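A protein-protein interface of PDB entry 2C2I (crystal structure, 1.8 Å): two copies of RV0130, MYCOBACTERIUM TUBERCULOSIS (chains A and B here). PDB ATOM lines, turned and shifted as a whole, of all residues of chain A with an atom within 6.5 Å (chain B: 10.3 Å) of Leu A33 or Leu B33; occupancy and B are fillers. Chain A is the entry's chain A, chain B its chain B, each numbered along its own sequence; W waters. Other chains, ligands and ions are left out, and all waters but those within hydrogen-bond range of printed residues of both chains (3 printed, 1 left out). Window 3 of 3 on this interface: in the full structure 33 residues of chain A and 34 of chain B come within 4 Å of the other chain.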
ATOM      1  N   GLN A  28     -15.851  17.706  42.482  1.00  0.00           N
ATOM      2  CA  GLN A  28     -16.877  16.701  42.209  1.00  0.00           C
ATOM      3  C   GLN A  28     -17.492  16.920  40.820  1.00  0.00           C
ATOM      4  O   GLN A  28     -17.776  15.957  40.104  1.00  0.00           O
ATOM      5  CB  GLN A  28     -17.951  16.693  43.302  1.00  0.00           C
ATOM      6  CG  GLN A  28     -18.930  15.547  43.148  1.00  0.00           C
ATOM      7  CD  GLN A  28     -18.284  14.182  43.344  1.00  0.00           C
ATOM      8  OE1 GLN A  28     -17.773  13.875  44.417  1.00  0.00           O
ATOM      9  NE2 GLN A  28     -18.341  13.344  42.307  1.00  0.00           N
ATOM     10  N   GLU A  29     -17.665  18.184  40.432  1.00  0.00           N
ATOM     11  CA  GLU A  29     -18.185  18.526  39.103  1.00  0.00           C
ATOM     12  C   GLU A  29     -17.313  17.917  38.004  1.00  0.00           C
ATOM     13  O   GLU A  29     -17.827  17.402  37.023  1.00  0.00           O
ATOM     14  CB  GLU A  29     -18.310  20.049  38.936  1.00  0.00           C
ATOM     15  CG  GLU A  29     -17.933  20.604  37.560  1.00  0.00           C
ATOM     16  CD  GLU A  29     -19.088  21.132  36.699  1.00  0.00           C
ATOM     17  OE1 GLU A  29     -18.853  22.145  36.003  1.00  0.00           O
ATOM     18  OE2 GLU A  29     -20.206  20.551  36.679  1.00  0.00           O
ATOM     19  N   GLU A  30     -15.992  17.988  38.178  1.00  0.00           N
ATOM     20  CA  GLU A  30     -15.071  17.427  37.184  1.00  0.00           C
ATOM     21  C   GLU A  30     -15.151  15.917  37.167  1.00  0.00           C
ATOM     22  O   GLU A  30     -15.070  15.304  36.090  1.00  0.00           O
ATOM     23  CB  GLU A  30     -13.638  17.876  37.455  1.00  0.00           C
ATOM     24  CG  GLU A  30     -13.443  19.374  37.255  1.00  0.00           C
ATOM     25  CD  GLU A  30     -12.069  19.839  37.706  1.00  0.00           C
ATOM     26  OE1 GLU A  30     -11.478  19.213  38.629  1.00  0.00           O
ATOM     27  OE2 GLU A  30     -11.575  20.817  37.111  1.00  0.00           O
ATOM     28  N   VAL A  31     -15.292  15.325  38.347  1.00  0.00           N
ATOM     29  CA  VAL A  31     -15.328  13.863  38.483  1.00  0.00           C
ATOM     30  C   VAL A  31     -16.597  13.319  37.815  1.00  0.00           C
ATOM     31  O   VAL A  31     -16.550  12.310  37.103  1.00  0.00           O
ATOM     32  CB  VAL A  31     -15.191  13.404  39.952  1.00  0.00           C
ATOM     33  CG1 VAL A  31     -15.386  11.888  40.086  1.00  0.00           C
ATOM     34  CG2 VAL A  31     -13.819  13.778  40.511  1.00  0.00           C
ATOM     35  N   ASN A  32     -17.714  14.022  38.036  1.00  0.00           N
ATOM     36  CA  ASN A  32     -18.997  13.735  37.353  1.00  0.00           C
ATOM     37  C   ASN A  32     -18.950  13.876  35.837  1.00  0.00           C
ATOM     38  O   ASN A  32     -19.493  13.031  35.122  1.00  0.00           O
ATOM     39  CB  ASN A  32     -20.100  14.638  37.913  1.00  0.00           C
ATOM     40  CG  ASN A  32     -20.344  14.417  39.388  1.00  0.00           C
ATOM     41  OD1 ASN A  32     -19.822  13.490  39.992  1.00  0.00           O
ATOM     42  ND2 ASN A  32     -21.143  15.296  39.984  1.00  0.00           N
ATOM     43  N   LEU A  33     -18.300  14.926  35.331  1.00  0.00           N
ATOM     44  CA  LEU A  33     -18.179  15.121  33.890  1.00  0.00           C
ATOM     45  C   LEU A  33     -17.346  13.977  33.308  1.00  0.00           C
ATOM     46  O   LEU A  33     -17.653  13.499  32.233  1.00  0.00           O
ATOM     47  CB  LEU A  33     -17.513  16.451  33.534  1.00  0.00           C
ATOM     48  CG  LEU A  33     -18.252  17.775  33.819  1.00  0.00           C
ATOM     49  CD1 LEU A  33     -17.380  18.987  33.539  1.00  0.00           C
ATOM     50  CD2 LEU A  33     -19.530  17.835  33.020  1.00  0.00           C
ATOM     51  N   PHE A  34     -16.302  13.569  34.039  1.00  0.00           N
ATOM     52  CA  PHE A  34     -15.435  12.462  33.612  1.00  0.00           C
ATOM     53  C   PHE A  34     -16.211  11.152  33.483  1.00  0.00           C
ATOM     54  O   PHE A  34     -16.039  10.390  32.508  1.00  0.00           O
ATOM     55  CB  PHE A  34     -14.258  12.275  34.566  1.00  0.00           C
ATOM     56  CG  PHE A  34     -13.157  11.405  33.991  1.00  0.00           C
ATOM     57  CD1 PHE A  34     -12.229  11.941  33.109  1.00  0.00           C
ATOM     58  CD2 PHE A  34     -13.076  10.051  34.327  1.00  0.00           C
ATOM     59  CE1 PHE A  34     -11.204  11.124  32.561  1.00  0.00           C
ATOM     60  CE2 PHE A  34     -12.065   9.221  33.782  1.00  0.00           C
ATOM     61  CZ  PHE A  34     -11.129   9.762  32.906  1.00  0.00           C
ATOM     62  N   ALA A  35     -17.024  10.886  34.504  1.00  0.00           N
ATOM     63  CA  ALA A  35     -17.924   9.755  34.532  1.00  0.00           C
ATOM     64  C   ALA A  35     -18.862   9.802  33.334  1.00  0.00           C
ATOM     65  O   ALA A  35     -19.045   8.801  32.673  1.00  0.00           O
ATOM     66  CB  ALA A  35     -18.729   9.739  35.861  1.00  0.00           C
ATOM     67  N   ASP A  36     -19.447  10.969  33.042  1.00  0.00           N
ATOM     68  CA  ASP A  36     -20.325  11.099  31.859  1.00  0.00           C
ATOM     69  C   ASP A  36     -19.578  10.863  30.543  1.00  0.00           C
ATOM     70  O   ASP A  36     -20.093  10.175  29.648  1.00  0.00           O
ATOM     71  CB  ASP A  36     -21.017  12.467  31.811  1.00  0.00           C
ATOM     72  CG  ASP A  36     -21.967  12.694  32.979  1.00  0.00           C
ATOM     73  OD1 ASP A  36     -22.395  11.724  33.644  1.00  0.00           O
ATOM     74  OD2 ASP A  36     -22.290  13.877  33.244  1.00  0.00           O
ATOM     75  N   ALA A  37     -18.378  11.441  30.432  1.00  0.00           N
ATOM     76  CA  ALA A  37     -17.562  11.309  29.230  1.00  0.00           C
ATOM     77  C   ALA A  37     -17.190   9.843  28.943  1.00  0.00           C
ATOM     78  O   ALA A  37     -17.182   9.417  27.789  1.00  0.00           O
ATOM     79  CB  ALA A  37     -16.309  12.162  29.346  1.00  0.00           C
ATOM     80  N   THR A  38     -16.879   9.090  29.991  1.00  0.00           N
ATOM     81  CA  THR A  38     -16.237   7.771  29.822  1.00  0.00           C
ATOM     82  C   THR A  38     -17.124   6.559  30.154  1.00  0.00           C
ATOM     83  O   THR A  38     -16.745   5.419  29.870  1.00  0.00           O
ATOM     84  CB  THR A  38     -14.964   7.667  30.704  1.00  0.00           C
ATOM     85  OG1 THR A  38     -15.331   7.747  32.083  1.00  0.00           O
ATOM     86  CG2 THR A  38     -13.949   8.790  30.375  1.00  0.00           C
ATOM     87  N   ILE B  26     -18.094   7.209  19.053  1.00  0.00           N
ATOM     88  CA  ILE B  26     -17.417   8.316  19.747  1.00  0.00           C
ATOM     89  C   ILE B  26     -18.115   9.603  19.347  1.00  0.00           C
ATOM     90  O   ILE B  26     -18.159   9.940  18.175  1.00  0.00           O
ATOM     91  CB  ILE B  26     -15.926   8.394  19.322  1.00  0.00           C
ATOM     92  CG1 ILE B  26     -15.207   7.084  19.655  1.00  0.00           C
ATOM     93  CG2 ILE B  26     -15.234   9.632  19.943  1.00  0.00           C
ATOM     94  CD1 ILE B  26     -15.092   6.792  21.160  1.00  0.00           C
ATOM     95  N   THR B  27     -18.642  10.339  20.322  1.00  0.00           N
ATOM     96  CA  THR B  27     -19.452  11.509  19.980  1.00  0.00           C
ATOM     97  C   THR B  27     -18.707  12.794  20.362  1.00  0.00           C
ATOM     98  O   THR B  27     -17.894  12.811  21.306  1.00  0.00           O
ATOM     99  CB  THR B  27     -20.805  11.516  20.708  1.00  0.00           C
ATOM    100  OG1 THR B  27     -20.573  11.626  22.117  1.00  0.00           O
ATOM    101  CG2 THR B  27     -21.636  10.217  20.385  1.00  0.00           C
ATOM    102  N   GLN B  28     -19.028  13.877  19.674  1.00  0.00           N
ATOM    103  CA  GLN B  28     -18.382  15.145  20.008  1.00  0.00           C
ATOM    104  C   GLN B  28     -18.699  15.586  21.422  1.00  0.00           C
ATOM    105  O   GLN B  28     -17.864  16.173  22.103  1.00  0.00           O
ATOM    106  CB  GLN B  28     -18.744  16.247  19.006  1.00  0.00           C
ATOM    107  CG  GLN B  28     -17.906  17.479  19.227  1.00  0.00           C
ATOM    108  CD  GLN B  28     -16.433  17.249  18.820  1.00  0.00           C
ATOM    109  OE1 GLN B  28     -16.133  16.820  17.687  1.00  0.00           O
ATOM    110  NE2 GLN B  28     -15.530  17.530  19.739  1.00  0.00           N
ATOM    111  N   GLU B  29     -19.906  15.301  21.890  1.00  0.00           N
ATOM    112  CA  GLU B  29     -20.248  15.745  23.231  1.00  0.00           C
ATOM    113  C   GLU B  29     -19.452  14.988  24.303  1.00  0.00           C
ATOM    114  O   GLU B  29     -19.080  15.560  25.313  1.00  0.00           O
ATOM    115  CB  GLU B  29     -21.776  15.750  23.485  1.00  0.00           C
ATOM    116  CG  GLU B  29     -22.452  14.393  23.496  1.00  0.00           C
ATOM    117  CD  GLU B  29     -22.921  13.935  22.127  1.00  0.00           C
ATOM    118  OE1 GLU B  29     -22.544  14.522  21.070  1.00  0.00           O
ATOM    119  OE2 GLU B  29     -23.683  12.937  22.116  1.00  0.00           O
ATOM    120  N   GLU B  30     -19.140  13.716  24.063  1.00  0.00           N
ATOM    121  CA  GLU B  30     -18.273  13.006  25.002  1.00  0.00           C
ATOM    122  C   GLU B  30     -16.860  13.581  24.991  1.00  0.00           C
ATOM    123  O   GLU B  30     -16.241  13.708  26.055  1.00  0.00           O
ATOM    124  CB  GLU B  30     -18.224  11.513  24.669  1.00  0.00           C
ATOM    125  CG  GLU B  30     -19.493  10.756  25.013  1.00  0.00           C
ATOM    126  CD  GLU B  30     -19.522   9.383  24.342  1.00  0.00           C
ATOM    127  OE1 GLU B  30     -18.840   9.184  23.296  1.00  0.00           O
ATOM    128  OE2 GLU B  30     -20.195   8.504  24.896  1.00  0.00           O
ATOM    129  N   VAL B  31     -16.358  13.891  23.798  1.00  0.00           N
ATOM    130  CA  VAL B  31     -14.997  14.451  23.649  1.00  0.00           C
ATOM    131  C   VAL B  31     -14.934  15.786  24.415  1.00  0.00           C
ATOM    132  O   VAL B  31     -14.005  16.020  25.175  1.00  0.00           O
ATOM    133  CB  VAL B  31     -14.581  14.613  22.171  1.00  0.00           C
ATOM    134  CG1 VAL B  31     -13.234  15.384  22.047  1.00  0.00           C
ATOM    135  CG2 VAL B  31     -14.460  13.243  21.480  1.00  0.00           C
ATOM    136  N   ASN B  32     -15.961  16.623  24.224  1.00  0.00           N
ATOM    137  CA  ASN B  32     -16.102  17.920  24.900  1.00  0.00           C
ATOM    138  C   ASN B  32     -16.192  17.812  26.422  1.00  0.00           C
ATOM    139  O   ASN B  32     -15.537  18.567  27.128  1.00  0.00           O
ATOM    140  CB  ASN B  32     -17.323  18.676  24.352  1.00  0.00           C
ATOM    141  CG  ASN B  32     -17.122  19.173  22.921  1.00  0.00           C
ATOM    142  OD1 ASN B  32     -16.042  19.032  22.342  1.00  0.00           O
ATOM    143  ND2 ASN B  32     -18.175  19.761  22.348  1.00  0.00           N
ATOM    144  N   LEU B  33     -16.994  16.866  26.917  1.00  0.00           N
ATOM    145  CA  LEU B  33     -17.056  16.564  28.331  1.00  0.00           C
ATOM    146  C   LEU B  33     -15.676  16.166  28.841  1.00  0.00           C
ATOM    147  O   LEU B  33     -15.285  16.560  29.939  1.00  0.00           O
ATOM    148  CB  LEU B  33     -18.032  15.418  28.608  1.00  0.00           C
ATOM    149  CG  LEU B  33     -19.519  15.762  28.490  1.00  0.00           C
ATOM    150  CD1 LEU B  33     -20.404  14.497  28.647  1.00  0.00           C
ATOM    151  CD2 LEU B  33     -19.869  16.827  29.523  1.00  0.00           C
ATOM    152  N   PHE B  34     -14.978  15.344  28.053  1.00  0.00           N
ATOM    153  CA  PHE B  34     -13.670  14.850  28.493  1.00  0.00           C
ATOM    154  C   PHE B  34     -12.686  16.019  28.622  1.00  0.00           C
ATOM    155  O   PHE B  34     -11.911  16.072  29.591  1.00  0.00           O
ATOM    156  CB  PHE B  34     -13.131  13.773  27.548  1.00  0.00           C
ATOM    157  CG  PHE B  34     -11.922  13.049  28.082  1.00  0.00           C
ATOM    158  CD1 PHE B  34     -12.066  11.941  28.901  1.00  0.00           C
ATOM    159  CD2 PHE B  34     -10.626  13.459  27.719  1.00  0.00           C
ATOM    160  CE1 PHE B  34     -10.911  11.246  29.405  1.00  0.00           C
ATOM    161  CE2 PHE B  34      -9.499  12.760  28.197  1.00  0.00           C
ATOM    162  CZ  PHE B  34      -9.650  11.667  29.030  1.00  0.00           C
ATOM    163  N   ALA B  35     -12.717  16.917  27.636  1.00  0.00           N
ATOM    164  CA  ALA B  35     -11.872  18.112  27.610  1.00  0.00           C
ATOM    165  C   ALA B  35     -12.170  18.996  28.837  1.00  0.00           C
ATOM    166  O   ALA B  35     -11.247  19.466  29.525  1.00  0.00           O
ATOM    167  CB  ALA B  35     -12.095  18.870  26.297  1.00  0.00           C
ATOM    168  N   ASP B  36     -13.462  19.184  29.121  1.00  0.00           N
ATOM    169  CA  ASP B  36     -13.911  19.969  30.285  1.00  0.00           C
ATOM    170  C   ASP B  36     -13.476  19.334  31.609  1.00  0.00           C
ATOM    171  O   ASP B  36     -13.058  20.023  32.526  1.00  0.00           O
ATOM    172  CB  ASP B  36     -15.447  20.148  30.269  1.00  0.00           C
ATOM    173  CG  ASP B  36     -15.925  21.021  29.108  1.00  0.00           C
ATOM    174  OD1 ASP B  36     -15.121  21.768  28.511  1.00  0.00           O
ATOM    175  OD2 ASP B  36     -17.130  20.977  28.792  1.00  0.00           O
ATOM    176  N   ALA B  37     -13.553  18.009  31.687  1.00  0.00           N
ATOM    177  CA  ALA B  37     -13.195  17.275  32.896  1.00  0.00           C
ATOM    178  C   ALA B  37     -11.690  17.365  33.191  1.00  0.00           C
ATOM    179  O   ALA B  37     -11.304  17.529  34.330  1.00  0.00           O
ATOM    180  CB  ALA B  37     -13.620  15.812  32.777  1.00  0.00           C
ATOM    181  N   THR B  38     -10.871  17.254  32.153  1.00  0.00           N
ATOM    182  CA  THR B  38      -9.415  17.082  32.316  1.00  0.00           C
ATOM    183  C   THR B  38      -8.562  18.312  31.992  1.00  0.00           C
ATOM    184  O   THR B  38      -7.362  18.331  32.292  1.00  0.00           O
ATOM    185  CB  THR B  38      -8.918  15.920  31.435  1.00  0.00           C
ATOM    186  OG1 THR B  38      -9.126  16.277  30.060  1.00  0.00           O
ATOM    187  CG2 THR B  38      -9.675  14.628  31.752  1.00  0.00           C
ATOM    188  N   GLY B  39      -9.158  19.333  31.392  1.00  0.00           N
ATOM    189  CA  GLY B  39      -8.417  20.536  31.031  1.00  0.00           C
ATOM    190  C   GLY B  39      -7.613  20.417  29.747  1.00  0.00           C
ATOM    191  O   GLY B  39      -6.763  21.268  29.461  1.00  0.00           O
ATOM    192  N   ASP B  40      -7.851  19.361  28.958  1.00  0.00           N
ATOM    193  CA  ASP B  40      -7.209  19.283  27.637  1.00  0.00           C
ATOM    194  C   ASP B  40      -8.208  19.709  26.567  1.00  0.00           C
ATOM    195  O   ASP B  40      -9.049  18.899  26.120  1.00  0.00           O
ATOM    196  CB  ASP B  40      -6.628  17.869  27.386  1.00  0.00           C
ATOM    197  CG  ASP B  40      -5.888  17.750  26.046  1.00  0.00           C
ATOM    198  OD1 ASP B  40      -5.967  18.655  25.202  1.00  0.00           O
ATOM    199  OD2 ASP B  40      -5.209  16.741  25.832  1.00  0.00           O
ATOM    200  N   HIS B  41      -8.145  20.991  26.186  1.00  0.00           N
ATOM    201  CA  HIS B  41      -8.985  21.509  25.098  1.00  0.00           C
ATOM    202  C   HIS B  41      -8.207  21.701  23.816  1.00  0.00           C
ATOM    203  O   HIS B  41      -8.460  22.637  23.059  1.00  0.00           O
ATOM    204  CB  HIS B  41      -9.707  22.806  25.510  1.00  0.00           C
ATOM    205  CG  HIS B  41     -10.608  22.645  26.700  1.00  0.00           C
ATOM    206  ND1 HIS B  41     -10.149  22.733  27.994  1.00  0.00           N
ATOM    207  CD2 HIS B  41     -11.936  22.389  26.790  1.00  0.00           C
ATOM    208  CE1 HIS B  41     -11.155  22.556  28.833  1.00  0.00           C
ATOM    209  NE2 HIS B  41     -12.252  22.343  28.126  1.00  0.00           N
ATOM    210  N   HIS B  45      -9.042  18.089  19.217  1.00  0.00           N
ATOM    211  CA  HIS B  45     -10.186  17.399  19.847  1.00  0.00           C
ATOM    212  C   HIS B  45     -11.495  18.190  19.802  1.00  0.00           C
ATOM    213  O   HIS B  45     -12.549  17.601  19.625  1.00  0.00           O
ATOM    214  CB  HIS B  45      -9.897  17.022  21.325  1.00  0.00           C
ATOM    215  CG  HIS B  45      -8.574  16.349  21.520  1.00  0.00           C
ATOM    216  ND1 HIS B  45      -8.273  15.134  20.947  1.00  0.00           N
ATOM    217  CD2 HIS B  45      -7.467  16.729  22.207  1.00  0.00           C
ATOM    218  CE1 HIS B  45      -7.030  14.799  21.260  1.00  0.00           C
ATOM    219  NE2 HIS B  45      -6.517  15.753  22.015  1.00  0.00           N
ATOM    220  N   VAL B  46     -11.422  19.517  19.933  1.00  0.00           N
ATOM    221  CA  VAL B  46     -12.607  20.305  20.321  1.00  0.00           C
ATOM    222  C   VAL B  46     -12.940  21.475  19.400  1.00  0.00           C
ATOM    223  O   VAL B  46     -13.929  22.176  19.634  1.00  0.00           O
ATOM    224  CB  VAL B  46     -12.525  20.802  21.803  1.00  0.00           C
ATOM    225  CG1 VAL B  46     -12.411  19.623  22.764  1.00  0.00           C
ATOM    226  CG2 VAL B  46     -11.359  21.793  22.015  1.00  0.00           C
ATOM    227  N   HIS B  62      -9.325  12.128  22.456  1.00  0.00           N
ATOM    228  CA  HIS B  62      -8.134  12.152  23.264  1.00  0.00           C
ATOM    229  C   HIS B  62      -7.706  10.703  23.459  1.00  0.00           C
ATOM    230  O   HIS B  62      -8.532   9.861  23.802  1.00  0.00           O
ATOM    231  CB  HIS B  62      -8.435  12.674  24.681  1.00  0.00           C
ATOM    232  CG  HIS B  62      -8.959  14.080  24.747  1.00  0.00           C
ATOM    233  ND1 HIS B  62     -10.278  14.407  24.488  1.00  0.00           N
ATOM    234  CD2 HIS B  62      -8.355  15.225  25.145  1.00  0.00           C
ATOM    235  CE1 HIS B  62     -10.445  15.709  24.667  1.00  0.00           C
ATOM    236  NE2 HIS B  62      -9.297  16.227  25.083  1.00  0.00           N
ATOM    237  N   MET B  65      -8.806   9.457  26.602  1.00  0.00           N
ATOM    238  CA  MET B  65     -10.211   9.068  26.690  1.00  0.00           C
ATOM    239  C   MET B  65     -10.398   7.665  26.157  1.00  0.00           C
ATOM    240  O   MET B  65     -11.035   6.865  26.801  1.00  0.00           O
ATOM    241  CB  MET B  65     -11.169  10.016  25.974  1.00  0.00           C
ATOM    242  CG  MET B  65     -12.633   9.566  26.211  1.00  0.00           C
ATOM    243  SD  MET B  65     -13.995  10.781  25.491  1.00  0.00           S
ATOM    244  CE  MET B  65     -13.409  11.052  24.372  1.00  0.00           C
ATOM    245  N   ALA B  68      -9.467   5.435  28.808  1.00  0.00           N
ATOM    246  CA  ALA B  68     -10.446   5.545  29.902  1.00  0.00           C
ATOM    247  C   ALA B  68     -11.793   4.880  29.594  1.00  0.00           C
ATOM    248  O   ALA B  68     -12.642   4.756  30.481  1.00  0.00           O
ATOM    249  CB  ALA B  68     -10.671   7.007  30.228  1.00  0.00           C
ATOM    250  N   LEU B  69     -12.008   4.494  28.330  1.00  0.00           N
ATOM    251  CA  LEU B  69     -13.186   3.702  27.971  1.00  0.00           C
ATOM    252  C   LEU B  69     -13.041   2.222  28.337  1.00  0.00           C
ATOM    253  O   LEU B  69     -14.011   1.456  28.209  1.00  0.00           O
ATOM    254  CB  LEU B  69     -13.490   3.828  26.473  1.00  0.00           C
ATOM    255  CG  LEU B  69     -13.988   5.155  25.910  1.00  0.00           C
ATOM    256  CD1 LEU B  69     -14.259   4.969  24.408  1.00  0.00           C
ATOM    257  CD2 LEU B  69     -15.259   5.606  26.654  1.00  0.00           C
ATOM    258  N   ARG B  72     -15.840   0.971  30.819  1.00  0.00           N
ATOM    259  CA  ARG B  72     -17.138   0.866  30.125  1.00  0.00           C
ATOM    260  C   ARG B  72     -17.207  -0.388  29.223  1.00  0.00           C
ATOM    261  O   ARG B  72     -18.179  -1.165  29.270  1.00  0.00           O
ATOM    262  CB  ARG B  72     -17.352   2.109  29.265  1.00  0.00           C
ATOM    263  CG  ARG B  72     -18.656   2.080  28.505  1.00  0.00           C
ATOM    264  CD  ARG B  72     -18.768   3.296  27.642  1.00  0.00           C
ATOM    265  NE  ARG B  72     -19.943   3.162  26.793  1.00  0.00           N
ATOM    266  CZ  ARG B  72     -20.245   3.986  25.806  1.00  0.00           C
ATOM    267  NH1 ARG B  72     -19.454   5.024  25.520  1.00  0.00           N
ATOM    268  NH2 ARG B  72     -21.367   3.777  25.122  1.00  0.00           N
ATOM    269  N   VAL B 102     -13.851  11.549  15.684  1.00  0.00           N
ATOM    270  CA  VAL B 102     -15.199  11.712  16.220  1.00  0.00           C
ATOM    271  C   VAL B 102     -16.181  11.210  15.147  1.00  0.00           C
ATOM    272  O   VAL B 102     -15.990  11.452  13.933  1.00  0.00           O
ATOM    273  CB  VAL B 102     -15.467  13.182  16.676  1.00  0.00           C
ATOM    274  CG1 VAL B 102     -16.946  13.419  16.891  1.00  0.00           C
ATOM    275  CG2 VAL B 102     -14.690  13.460  17.987  1.00  0.00           C
HETATM  276  O   HOH W   1     -12.961   6.175  32.819  1.00  0.00           O
HETATM  277  O   HOH W   2      -9.738  18.025  36.569  1.00  0.00           O
HETATM  278  O   HOH W   3     -14.954   3.751  31.120  1.00  0.00           O
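O of Phe B34 sits at hydrogen-bond distance from OG1 of Thr B38 (2.8 Å). NE2 of His B41 lies within hydrogen-bond range of OD1 of Asp B36 (3.0 Å). O of Phe A34 sits at hydrogen-bond distance from OG1 of Thr A38 (2.8 Å). The side-chain carboxylate (OE2) of Glu B30 is in salt-bridge range of the guanidinium group (NH1) of Arg B72 (3.6 Å). The side-chain hydroxyl (OG1) of Thr B27 sits at hydrogen-bond distance from the backbone NH (N) of Glu B30, at 3.2 Å.
Among the printed residues, pairs that only touch across the chains: Phe A34 with Phe B34, Thr A38 with Arg B72, Thr A38 with Leu B69, Ala A37 with Glu B30, Glu A30 with Ala B37, Leu A33 with Leu B33, Ala A37 with Phe B34, Phe A34 with Ala B37, Thr A38 with Ala B68, Ala A37 with Leu B33, Asp A36 with Leu B33, Phe A34 with Ala B68, Phe A34 with Thr B38, Thr A38 with Phe B34 and Leu A33 with Asp B36.
No residue of chain B comes within 4 Å of Glu A29. No residue of chain B comes within 4 Å of Asn A32. Of the printed residues of chain B, Leu A33 touches Leu B33 (3.7 Å) and Asp B36 (3.97 Å). Of the printed residues of chain B, Asp A36 touches Leu B33. Printed residues of chain B within 4 Å of Ala A37: Glu B30, Leu B33 and Phe B34. Of the printed residues of chain A, Glu B30 touches Ala A37. Of chain A, only Leu A33 (3.7 Å), Asp A36 (3.8 Å) and Ala A37 (3.8 Å) come within 4 Å of Leu B33. Printed residues of chain A within 4 Å of Phe B34: Phe A34 (3.2 Å), Ala A37 (3.7 Å) and Thr A38 (3.96 Å). The nearest residue of chain A that does not touch Leu B33 is Phe A34 (5.2 Å).
Hydrophobic or aromatic side chains of chain B that line the printed part of chain A: Leu B33, Phe B34, Ala B37, Ala B68 and Leu B69. Of the 11 printed residues of chain A, 6 touch a printed residue of chain B. Printed residues of chain A that touch a printed residue of chain B: Glu A30, Leu A33, Phe A34, Asp A36, Ala A37 and Thr A38. Among the printed residues, 15 pairs touch across the chains. Among the printed residues, no Asp or Glu carboxylate lies within 4 Å of a Lys or Arg side-chain nitrogen of the other chain.
Leu A33 touches its own counterpart, Leu B33. Phe A34 touches its own counterpart, Phe B34. Phe A34 touches Thr B38, and with the chains exchanged Thr A38 touches Phe B34. Ala A37 touches Leu B33, but with the chains exchanged Leu A33 does not touch Ala B37 (4.02 Å).
Water W3 lies within hydrogen-bond range of O of Ala B68 (2.6 Å), O of Thr A38 (2.7 Å) and N of Arg B72 (2.9 Å). Water W1 lies within hydrogen-bond range of O of Ala B68 and OG1 of Thr A38. Water W2 bridges the backbone carbonyl oxygen of Ala B37 and the side-chain carboxylate of Glu A30.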
